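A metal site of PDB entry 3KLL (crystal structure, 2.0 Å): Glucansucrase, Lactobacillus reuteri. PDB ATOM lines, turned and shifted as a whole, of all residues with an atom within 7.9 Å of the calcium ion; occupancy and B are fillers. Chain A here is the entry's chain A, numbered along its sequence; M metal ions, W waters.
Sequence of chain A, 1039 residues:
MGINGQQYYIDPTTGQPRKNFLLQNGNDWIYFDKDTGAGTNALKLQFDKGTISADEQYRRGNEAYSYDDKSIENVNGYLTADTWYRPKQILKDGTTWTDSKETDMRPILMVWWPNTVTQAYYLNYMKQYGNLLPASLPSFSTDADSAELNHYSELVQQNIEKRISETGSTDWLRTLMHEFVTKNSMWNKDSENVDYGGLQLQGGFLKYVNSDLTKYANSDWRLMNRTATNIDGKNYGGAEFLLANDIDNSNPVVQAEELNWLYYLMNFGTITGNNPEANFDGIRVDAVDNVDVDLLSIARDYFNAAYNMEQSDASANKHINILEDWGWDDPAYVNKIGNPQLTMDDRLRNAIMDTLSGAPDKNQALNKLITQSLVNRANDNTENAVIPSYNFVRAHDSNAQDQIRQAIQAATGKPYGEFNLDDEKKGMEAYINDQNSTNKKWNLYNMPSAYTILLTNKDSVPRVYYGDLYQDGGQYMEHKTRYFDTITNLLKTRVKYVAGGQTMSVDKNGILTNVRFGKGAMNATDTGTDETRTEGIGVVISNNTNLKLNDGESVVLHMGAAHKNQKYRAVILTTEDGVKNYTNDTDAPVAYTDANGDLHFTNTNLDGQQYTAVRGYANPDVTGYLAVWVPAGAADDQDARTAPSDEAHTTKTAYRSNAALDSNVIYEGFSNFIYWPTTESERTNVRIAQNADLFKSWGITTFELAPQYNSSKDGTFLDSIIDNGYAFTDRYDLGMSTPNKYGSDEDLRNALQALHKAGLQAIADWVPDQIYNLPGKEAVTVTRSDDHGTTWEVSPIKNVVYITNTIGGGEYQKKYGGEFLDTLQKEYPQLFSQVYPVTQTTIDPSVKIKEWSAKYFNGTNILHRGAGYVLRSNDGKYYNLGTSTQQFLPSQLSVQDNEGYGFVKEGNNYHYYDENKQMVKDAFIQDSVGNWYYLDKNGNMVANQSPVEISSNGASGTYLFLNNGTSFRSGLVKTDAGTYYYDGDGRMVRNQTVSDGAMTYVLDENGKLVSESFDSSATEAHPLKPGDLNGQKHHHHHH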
ATOM      1  N   LEU A 223       0.577   8.912  -5.434  1.00  0.00           N
ATOM      2  CA  LEU A 223       1.100   8.720  -6.791  1.00  0.00           C
ATOM      3  C   LEU A 223       0.174   7.745  -7.532  1.00  0.00           C
ATOM      4  O   LEU A 223       0.123   6.545  -7.204  1.00  0.00           O
ATOM      5  CB  LEU A 223       2.574   8.229  -6.791  1.00  0.00           C
ATOM      6  CG  LEU A 223       3.587   8.914  -5.884  1.00  0.00           C
ATOM      7  CD1 LEU A 223       4.973   8.245  -6.012  1.00  0.00           C
ATOM      8  CD2 LEU A 223       3.649  10.408  -6.211  1.00  0.00           C
ATOM      9  N   MET A 224      -0.547   8.264  -8.514  1.00  0.00           N
ATOM     10  CA  MET A 224      -1.649   7.528  -9.132  1.00  0.00           C
ATOM     11  C   MET A 224      -1.277   6.962 -10.489  1.00  0.00           C
ATOM     12  O   MET A 224      -0.445   7.567 -11.212  1.00  0.00           O
ATOM     13  CB  MET A 224      -2.863   8.445  -9.235  1.00  0.00           C
ATOM     14  CG  MET A 224      -3.449   8.743  -7.805  1.00  0.00           C
ATOM     15  SD  MET A 224      -4.971   9.862  -8.017  1.00  0.00           S
ATOM     16  CE  MET A 224      -4.108  11.316  -9.019  1.00  0.00           C
ATOM     17  N   ASN A 225      -1.872   5.812 -10.836  1.00  0.00           N
ATOM     18  CA  ASN A 225      -1.759   5.241 -12.195  1.00  0.00           C
ATOM     19  C   ASN A 225      -0.351   4.754 -12.490  1.00  0.00           C
ATOM     20  O   ASN A 225       0.034   4.682 -13.664  1.00  0.00           O
ATOM     21  CB  ASN A 225      -2.145   6.231 -13.350  1.00  0.00           C
ATOM     22  CG  ASN A 225      -3.341   7.111 -13.054  1.00  0.00           C
ATOM     23  OD1 ASN A 225      -4.424   6.638 -12.623  1.00  0.00           O
ATOM     24  ND2 ASN A 225      -3.181   8.401 -13.332  1.00  0.00           N
ATOM     25  N   GLY A 238      -2.440   2.449 -16.197  1.00  0.00           N
ATOM     26  CA  GLY A 238      -3.827   1.970 -15.979  1.00  0.00           C
ATOM     27  C   GLY A 238      -4.596   2.848 -15.003  1.00  0.00           C
ATOM     28  O   GLY A 238      -4.009   3.669 -14.316  1.00  0.00           O
ATOM     29  N   ALA A 239      -5.910   2.684 -14.901  1.00  0.00           N
ATOM     30  CA  ALA A 239      -6.697   3.559 -14.039  1.00  0.00           C
ATOM     31  C   ALA A 239      -6.539   3.300 -12.554  1.00  0.00           C
ATOM     32  O   ALA A 239      -6.888   2.215 -12.055  1.00  0.00           O
ATOM     33  CB  ALA A 239      -8.176   3.512 -14.449  1.00  0.00           C
ATOM     34  N   GLU A 240      -6.110   4.326 -11.818  1.00  0.00           N
ATOM     35  CA  GLU A 240      -5.908   4.189 -10.398  1.00  0.00           C
ATOM     36  C   GLU A 240      -7.223   3.876  -9.682  1.00  0.00           C
ATOM     37  O   GLU A 240      -7.239   3.053  -8.745  1.00  0.00           O
ATOM     38  CB  GLU A 240      -5.315   5.452  -9.820  1.00  0.00           C
ATOM     39  CG  GLU A 240      -4.931   5.313  -8.365  1.00  0.00           C
ATOM     40  CD  GLU A 240      -3.882   4.274  -8.120  1.00  0.00           C
ATOM     41  OE1 GLU A 240      -2.723   4.345  -8.694  1.00  0.00           O
ATOM     42  OE2 GLU A 240      -4.175   3.391  -7.294  1.00  0.00           O
ATOM     43  N   PHE A 241      -8.284   4.535 -10.147  1.00  0.00           N
ATOM     44  CA  PHE A 241      -9.600   4.429  -9.525  1.00  0.00           C
ATOM     45  C   PHE A 241     -10.440   3.345 -10.161  1.00  0.00           C
ATOM     46  O   PHE A 241     -10.490   3.216 -11.377  1.00  0.00           O
ATOM     47  CB  PHE A 241     -10.354   5.736  -9.601  1.00  0.00           C
ATOM     48  CG  PHE A 241      -9.766   6.837  -8.760  1.00  0.00           C
ATOM     49  CD1 PHE A 241      -9.773   6.747  -7.371  1.00  0.00           C
ATOM     50  CD2 PHE A 241      -9.212   7.960  -9.366  1.00  0.00           C
ATOM     51  CE1 PHE A 241      -9.238   7.765  -6.588  1.00  0.00           C
ATOM     52  CE2 PHE A 241      -8.678   8.967  -8.592  1.00  0.00           C
ATOM     53  CZ  PHE A 241      -8.698   8.888  -7.213  1.00  0.00           C
ATOM     54  N   LEU A 242     -11.133   2.577  -9.323  1.00  0.00           N
ATOM     55  CA  LEU A 242     -11.910   1.473  -9.791  1.00  0.00           C
ATOM     56  C   LEU A 242     -13.257   1.444  -9.011  1.00  0.00           C
ATOM     57  O   LEU A 242     -14.320   1.609  -9.617  1.00  0.00           O
ATOM     58  CB  LEU A 242     -11.133   0.162  -9.537  1.00  0.00           C
ATOM     59  CG  LEU A 242     -11.787  -1.182  -9.873  1.00  0.00           C
ATOM     60  CD1 LEU A 242     -12.250  -1.221 -11.334  1.00  0.00           C
ATOM     61  CD2 LEU A 242     -10.814  -2.291  -9.585  1.00  0.00           C
ATOM     62  N   LEU A 243     -13.183   1.259  -7.688  1.00  0.00           N
ATOM     63  CA  LEU A 243     -14.383   1.051  -6.819  1.00  0.00           C
ATOM     64  C   LEU A 243     -14.140   1.589  -5.428  1.00  0.00           C
ATOM     65  O   LEU A 243     -13.021   1.537  -4.913  1.00  0.00           O
ATOM     66  CB  LEU A 243     -14.689  -0.459  -6.695  1.00  0.00           C
ATOM     67  CG  LEU A 243     -15.322  -1.150  -7.920  1.00  0.00           C
ATOM     68  CD1 LEU A 243     -15.059  -2.672  -7.898  1.00  0.00           C
ATOM     69  CD2 LEU A 243     -16.821  -0.885  -8.022  1.00  0.00           C
ATOM     70  N   ASN A 245     -13.453   2.964  -1.796  1.00  0.00           N
ATOM     71  CA  ASN A 245     -12.384   3.766  -1.240  1.00  0.00           C
ATOM     72  C   ASN A 245     -11.030   3.295  -1.756  1.00  0.00           C
ATOM     73  O   ASN A 245     -10.516   2.241  -1.383  1.00  0.00           O
ATOM     74  CB  ASN A 245     -12.419   3.777   0.289  1.00  0.00           C
ATOM     75  CG  ASN A 245     -13.757   4.272   0.828  1.00  0.00           C
ATOM     76  OD1 ASN A 245     -14.083   5.465   0.800  1.00  0.00           O
ATOM     77  ND2 ASN A 245     -14.554   3.329   1.295  1.00  0.00           N
ATOM     78  N   ASP A 246     -10.435   4.088  -2.617  1.00  0.00           N
ATOM     79  CA  ASP A 246      -9.189   3.655  -3.225  1.00  0.00           C
ATOM     80  C   ASP A 246      -8.002   3.793  -2.315  1.00  0.00           C
ATOM     81  O   ASP A 246      -7.616   4.937  -1.958  1.00  0.00           O
ATOM     82  CB  ASP A 246      -8.937   4.409  -4.533  1.00  0.00           C
ATOM     83  CG  ASP A 246      -7.948   3.695  -5.391  1.00  0.00           C
ATOM     84  OD1 ASP A 246      -8.298   2.578  -5.822  1.00  0.00           O
ATOM     85  OD2 ASP A 246      -6.826   4.241  -5.663  1.00  0.00           O
ATOM     86  N   ILE A 247      -7.380   2.657  -1.953  1.00  0.00           N
ATOM     87  CA  ILE A 247      -6.201   2.652  -1.082  1.00  0.00           C
ATOM     88  C   ILE A 247      -4.995   3.287  -1.809  1.00  0.00           C
ATOM     89  O   ILE A 247      -4.748   2.966  -2.949  1.00  0.00           O
ATOM     90  CB  ILE A 247      -5.839   1.232  -0.643  1.00  0.00           C
ATOM     91  CG1 ILE A 247      -6.996   0.627   0.206  1.00  0.00           C
ATOM     92  CG2 ILE A 247      -4.644   1.251   0.252  1.00  0.00           C
ATOM     93  CD1 ILE A 247      -6.733  -0.829   0.618  1.00  0.00           C
ATOM     94  N   ASP A 248      -4.303   4.207  -1.171  1.00  0.00           N
ATOM     95  CA  ASP A 248      -3.079   4.783  -1.752  1.00  0.00           C
ATOM     96  C   ASP A 248      -1.880   3.833  -1.530  1.00  0.00           C
ATOM     97  O   ASP A 248      -1.171   3.913  -0.531  1.00  0.00           O
ATOM     98  CB  ASP A 248      -2.806   6.149  -1.140  1.00  0.00           C
ATOM     99  CG  ASP A 248      -1.493   6.767  -1.676  1.00  0.00           C
ATOM    100  OD1 ASP A 248      -0.966   6.288  -2.700  1.00  0.00           O
ATOM    101  OD2 ASP A 248      -1.007   7.719  -1.050  1.00  0.00           O
ATOM    102  N   ASN A 249      -1.698   2.893  -2.437  1.00  0.00           N
ATOM    103  CA  ASN A 249      -0.617   1.927  -2.329  1.00  0.00           C
ATOM    104  C   ASN A 249       0.732   2.500  -2.785  1.00  0.00           C
ATOM    105  O   ASN A 249       1.732   1.768  -2.833  1.00  0.00           O
ATOM    106  CB  ASN A 249      -0.946   0.664  -3.110  1.00  0.00           C
ATOM    107  CG  ASN A 249      -2.101  -0.118  -2.483  1.00  0.00           C
ATOM    108  OD1 ASN A 249      -3.233  -0.205  -3.029  1.00  0.00           O
ATOM    109  ND2 ASN A 249      -1.825  -0.685  -1.329  1.00  0.00           N
ATOM    110  N   ALA A 287      -6.791  -6.785  -9.345  1.00  0.00           N
ATOM    111  CA  ALA A 287      -6.787  -5.410  -9.873  1.00  0.00           C
ATOM    112  C   ALA A 287      -5.389  -4.837 -10.104  1.00  0.00           C
ATOM    113  O   ALA A 287      -5.091  -3.705  -9.706  1.00  0.00           O
ATOM    114  CB  ALA A 287      -7.625  -4.462  -8.968  1.00  0.00           C
ATOM    115  N   VAL A 288      -4.525  -5.661 -10.685  1.00  0.00           N
ATOM    116  CA  VAL A 288      -3.128  -5.253 -10.873  1.00  0.00           C
ATOM    117  C   VAL A 288      -3.030  -3.855 -11.537  1.00  0.00           C
ATOM    118  O   VAL A 288      -2.303  -2.991 -11.038  1.00  0.00           O
ATOM    119  CB  VAL A 288      -2.315  -6.277 -11.672  1.00  0.00           C
ATOM    120  CG1 VAL A 288      -0.937  -5.677 -12.098  1.00  0.00           C
ATOM    121  CG2 VAL A 288      -2.110  -7.548 -10.882  1.00  0.00           C
ATOM    122  N   ASP A 289      -3.729  -3.635 -12.643  1.00  0.00           N
ATOM    123  CA  ASP A 289      -3.608  -2.350 -13.374  1.00  0.00           C
ATOM    124  C   ASP A 289      -4.304  -1.145 -12.693  1.00  0.00           C
ATOM    125  O   ASP A 289      -4.474  -0.088 -13.288  1.00  0.00           O
ATOM    126  CB  ASP A 289      -4.054  -2.505 -14.822  1.00  0.00           C
ATOM    127  CG  ASP A 289      -3.188  -3.494 -15.594  1.00  0.00           C
ATOM    128  OD1 ASP A 289      -2.031  -3.708 -15.158  1.00  0.00           O
ATOM    129  OD2 ASP A 289      -3.649  -4.077 -16.601  1.00  0.00           O
ATOM    130  N   ASN A 290      -4.659  -1.315 -11.422  1.00  0.00           N
ATOM    131  CA  ASN A 290      -5.321  -0.227 -10.672  1.00  0.00           C
ATOM    132  C   ASN A 290      -4.636   0.144  -9.384  1.00  0.00           C
ATOM    133  O   ASN A 290      -5.236   0.824  -8.500  1.00  0.00           O
ATOM    134  CB  ASN A 290      -6.807  -0.611 -10.385  1.00  0.00           C
ATOM    135  CG  ASN A 290      -7.498  -1.210 -11.577  1.00  0.00           C
ATOM    136  OD1 ASN A 290      -7.729  -2.414 -11.635  1.00  0.00           O
ATOM    137  ND2 ASN A 290      -7.848  -0.359 -12.537  1.00  0.00           N
ATOM    138  N   VAL A 291      -3.400  -0.340  -9.228  1.00  0.00           N
ATOM    139  CA  VAL A 291      -2.604  -0.060  -8.039  1.00  0.00           C
ATOM    140  C   VAL A 291      -1.140   0.236  -8.484  1.00  0.00           C
ATOM    141  O   VAL A 291      -0.734  -0.145  -9.580  1.00  0.00           O
ATOM    142  CB  VAL A 291      -2.569  -1.252  -7.047  1.00  0.00           C
ATOM    143  CG1 VAL A 291      -4.024  -1.655  -6.608  1.00  0.00           C
ATOM    144  CG2 VAL A 291      -1.840  -2.451  -7.631  1.00  0.00           C
ATOM    145  N   ASP A 292      -0.403   0.868  -7.586  1.00  0.00           N
ATOM    146  CA  ASP A 292       1.056   1.023  -7.692  1.00  0.00           C
ATOM    147  C   ASP A 292       1.754  -0.341  -7.849  1.00  0.00           C
ATOM    148  O   ASP A 292       1.679  -1.228  -6.980  1.00  0.00           O
ATOM    149  CB  ASP A 292       1.561   1.798  -6.468  1.00  0.00           C
ATOM    150  CG  ASP A 292       3.072   1.957  -6.443  1.00  0.00           C
ATOM    151  OD1 ASP A 292       3.727   1.658  -7.484  1.00  0.00           O
ATOM    152  OD2 ASP A 292       3.587   2.369  -5.374  1.00  0.00           O
ATOM    153  N   PRO A 768      -5.547  -5.512  -2.640  1.00  0.00           N
ATOM    154  CA  PRO A 768      -5.066  -4.264  -2.068  1.00  0.00           C
ATOM    155  C   PRO A 768      -5.725  -3.011  -2.665  1.00  0.00           C
ATOM    156  O   PRO A 768      -5.434  -1.901  -2.204  1.00  0.00           O
ATOM    157  CB  PRO A 768      -3.557  -4.283  -2.432  1.00  0.00           C
ATOM    158  CG  PRO A 768      -3.522  -5.024  -3.752  1.00  0.00           C
ATOM    159  CD  PRO A 768      -4.488  -6.196  -3.402  1.00  0.00           C
ATOM    160  N   ASP A 769      -6.546  -3.131  -3.696  1.00  0.00           N
ATOM    161  CA  ASP A 769      -7.055  -1.888  -4.341  1.00  0.00           C
ATOM    162  C   ASP A 769      -7.919  -0.982  -3.447  1.00  0.00           C
ATOM    163  O   ASP A 769      -7.793   0.256  -3.467  1.00  0.00           O
ATOM    164  CB  ASP A 769      -7.812  -2.193  -5.606  1.00  0.00           C
ATOM    165  CG  ASP A 769      -8.219  -0.935  -6.344  1.00  0.00           C
ATOM    166  OD1 ASP A 769      -7.309  -0.226  -6.850  1.00  0.00           O
ATOM    167  OD2 ASP A 769      -9.446  -0.651  -6.429  1.00  0.00           O
ATOM    168  N   GLN A 770      -8.851  -1.588  -2.693  1.00  0.00           N
ATOM    169  CA  GLN A 770      -9.884  -0.752  -2.075  1.00  0.00           C
ATOM    170  C   GLN A 770     -10.499  -1.400  -0.849  1.00  0.00           C
ATOM    171  O   GLN A 770     -10.282  -2.588  -0.562  1.00  0.00           O
ATOM    172  CB  GLN A 770     -11.010  -0.402  -3.081  1.00  0.00           C
ATOM    173  CG  GLN A 770     -12.091  -1.563  -3.358  1.00  0.00           C
ATOM    174  CD  GLN A 770     -11.576  -2.664  -4.333  1.00  0.00           C
ATOM    175  OE1 GLN A 770     -11.055  -2.354  -5.423  1.00  0.00           O
ATOM    176  NE2 GLN A 770     -11.756  -3.958  -3.958  1.00  0.00           N
ATOM    177  N   ASP A 787     -11.181   8.262 -14.036  1.00  0.00           N
ATOM    178  CA  ASP A 787     -10.606   7.072 -13.421  1.00  0.00           C
ATOM    179  C   ASP A 787      -9.067   7.114 -13.284  1.00  0.00           C
ATOM    180  O   ASP A 787      -8.473   6.258 -12.619  1.00  0.00           O
ATOM    181  CB  ASP A 787     -11.093   5.772 -14.096  1.00  0.00           C
ATOM    182  CG  ASP A 787     -10.665   5.623 -15.576  1.00  0.00           C
ATOM    183  OD1 ASP A 787      -9.744   6.323 -16.085  1.00  0.00           O
ATOM    184  OD2 ASP A 787     -11.238   4.727 -16.243  1.00  0.00           O
ATOM    185  N   ASN A 858      -6.539   7.466  -1.999  1.00  0.00           N
ATOM    186  CA  ASN A 858      -6.464   8.322  -3.187  1.00  0.00           C
ATOM    187  C   ASN A 858      -7.729   9.087  -3.476  1.00  0.00           C
ATOM    188  O   ASN A 858      -7.681  10.177  -4.027  1.00  0.00           O
ATOM    189  CB  ASN A 858      -6.147   7.474  -4.419  1.00  0.00           C
ATOM    190  CG  ASN A 858      -4.682   7.028  -4.439  1.00  0.00           C
ATOM    191  OD1 ASN A 858      -3.831   7.749  -3.957  1.00  0.00           O
ATOM    192  ND2 ASN A 858      -4.407   5.818  -4.937  1.00  0.00           N
HETATM  193 CA    CA M   1      -6.225   2.092  -7.017  1.00  0.00          CA
HETATM  194  O   HOH W   1      -5.657   1.233  -4.697  1.00  0.00           O
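The backbone carbonyl oxygen of Ala 239 is in hydrogen-bond range of the side-chain amide nitrogen of Asn 290 (2.8 Å). The side-chain amide nitrogen of Asn 858 sits close to the side-chain carboxylate of Glu 240. The side-chain carboxylate (OE1) of Glu 240 lies within hydrogen-bond range of the backbone NH (N) of Asn 225 (2.7 Å). The backbone NH (N) of Glu 240 sits at hydrogen-bond distance from the backbone carbonyl oxygen (O) of Asp 787, at 3.2 Å. The backbone NH (N) of Asn 858 lies within hydrogen-bond range of the backbone carbonyl oxygen (O) of Asp 246, at 2.7 Å. The backbone NH (N) of Ile 247 lies within hydrogen-bond range of the backbone carbonyl oxygen (O) of Asp 769 (2.9 Å). The side-chain amide oxygen of Gln 770 lies close to the side-chain carboxylate of Asp 769, at 2.5 Å.
The calcium ion is bound by O of Asn 290 (2.2 Å), O of Glu 240 (2.2 Å), OD1 of Asp 246 (2.4 Å), OE2 of Glu 240 (2.4 Å), water W1 (2.5 Å), OD1 of Asp 769 (2.6 Å) and OD2 of Asp 246 (2.6 Å).
Four residues have an atom within 4 Å of the calcium ion: Glu 240, Asp 246, Asn 290 and Asp 769. The nearest printed residue that does not touch the calcium ion is Val 291 (4.3 Å).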
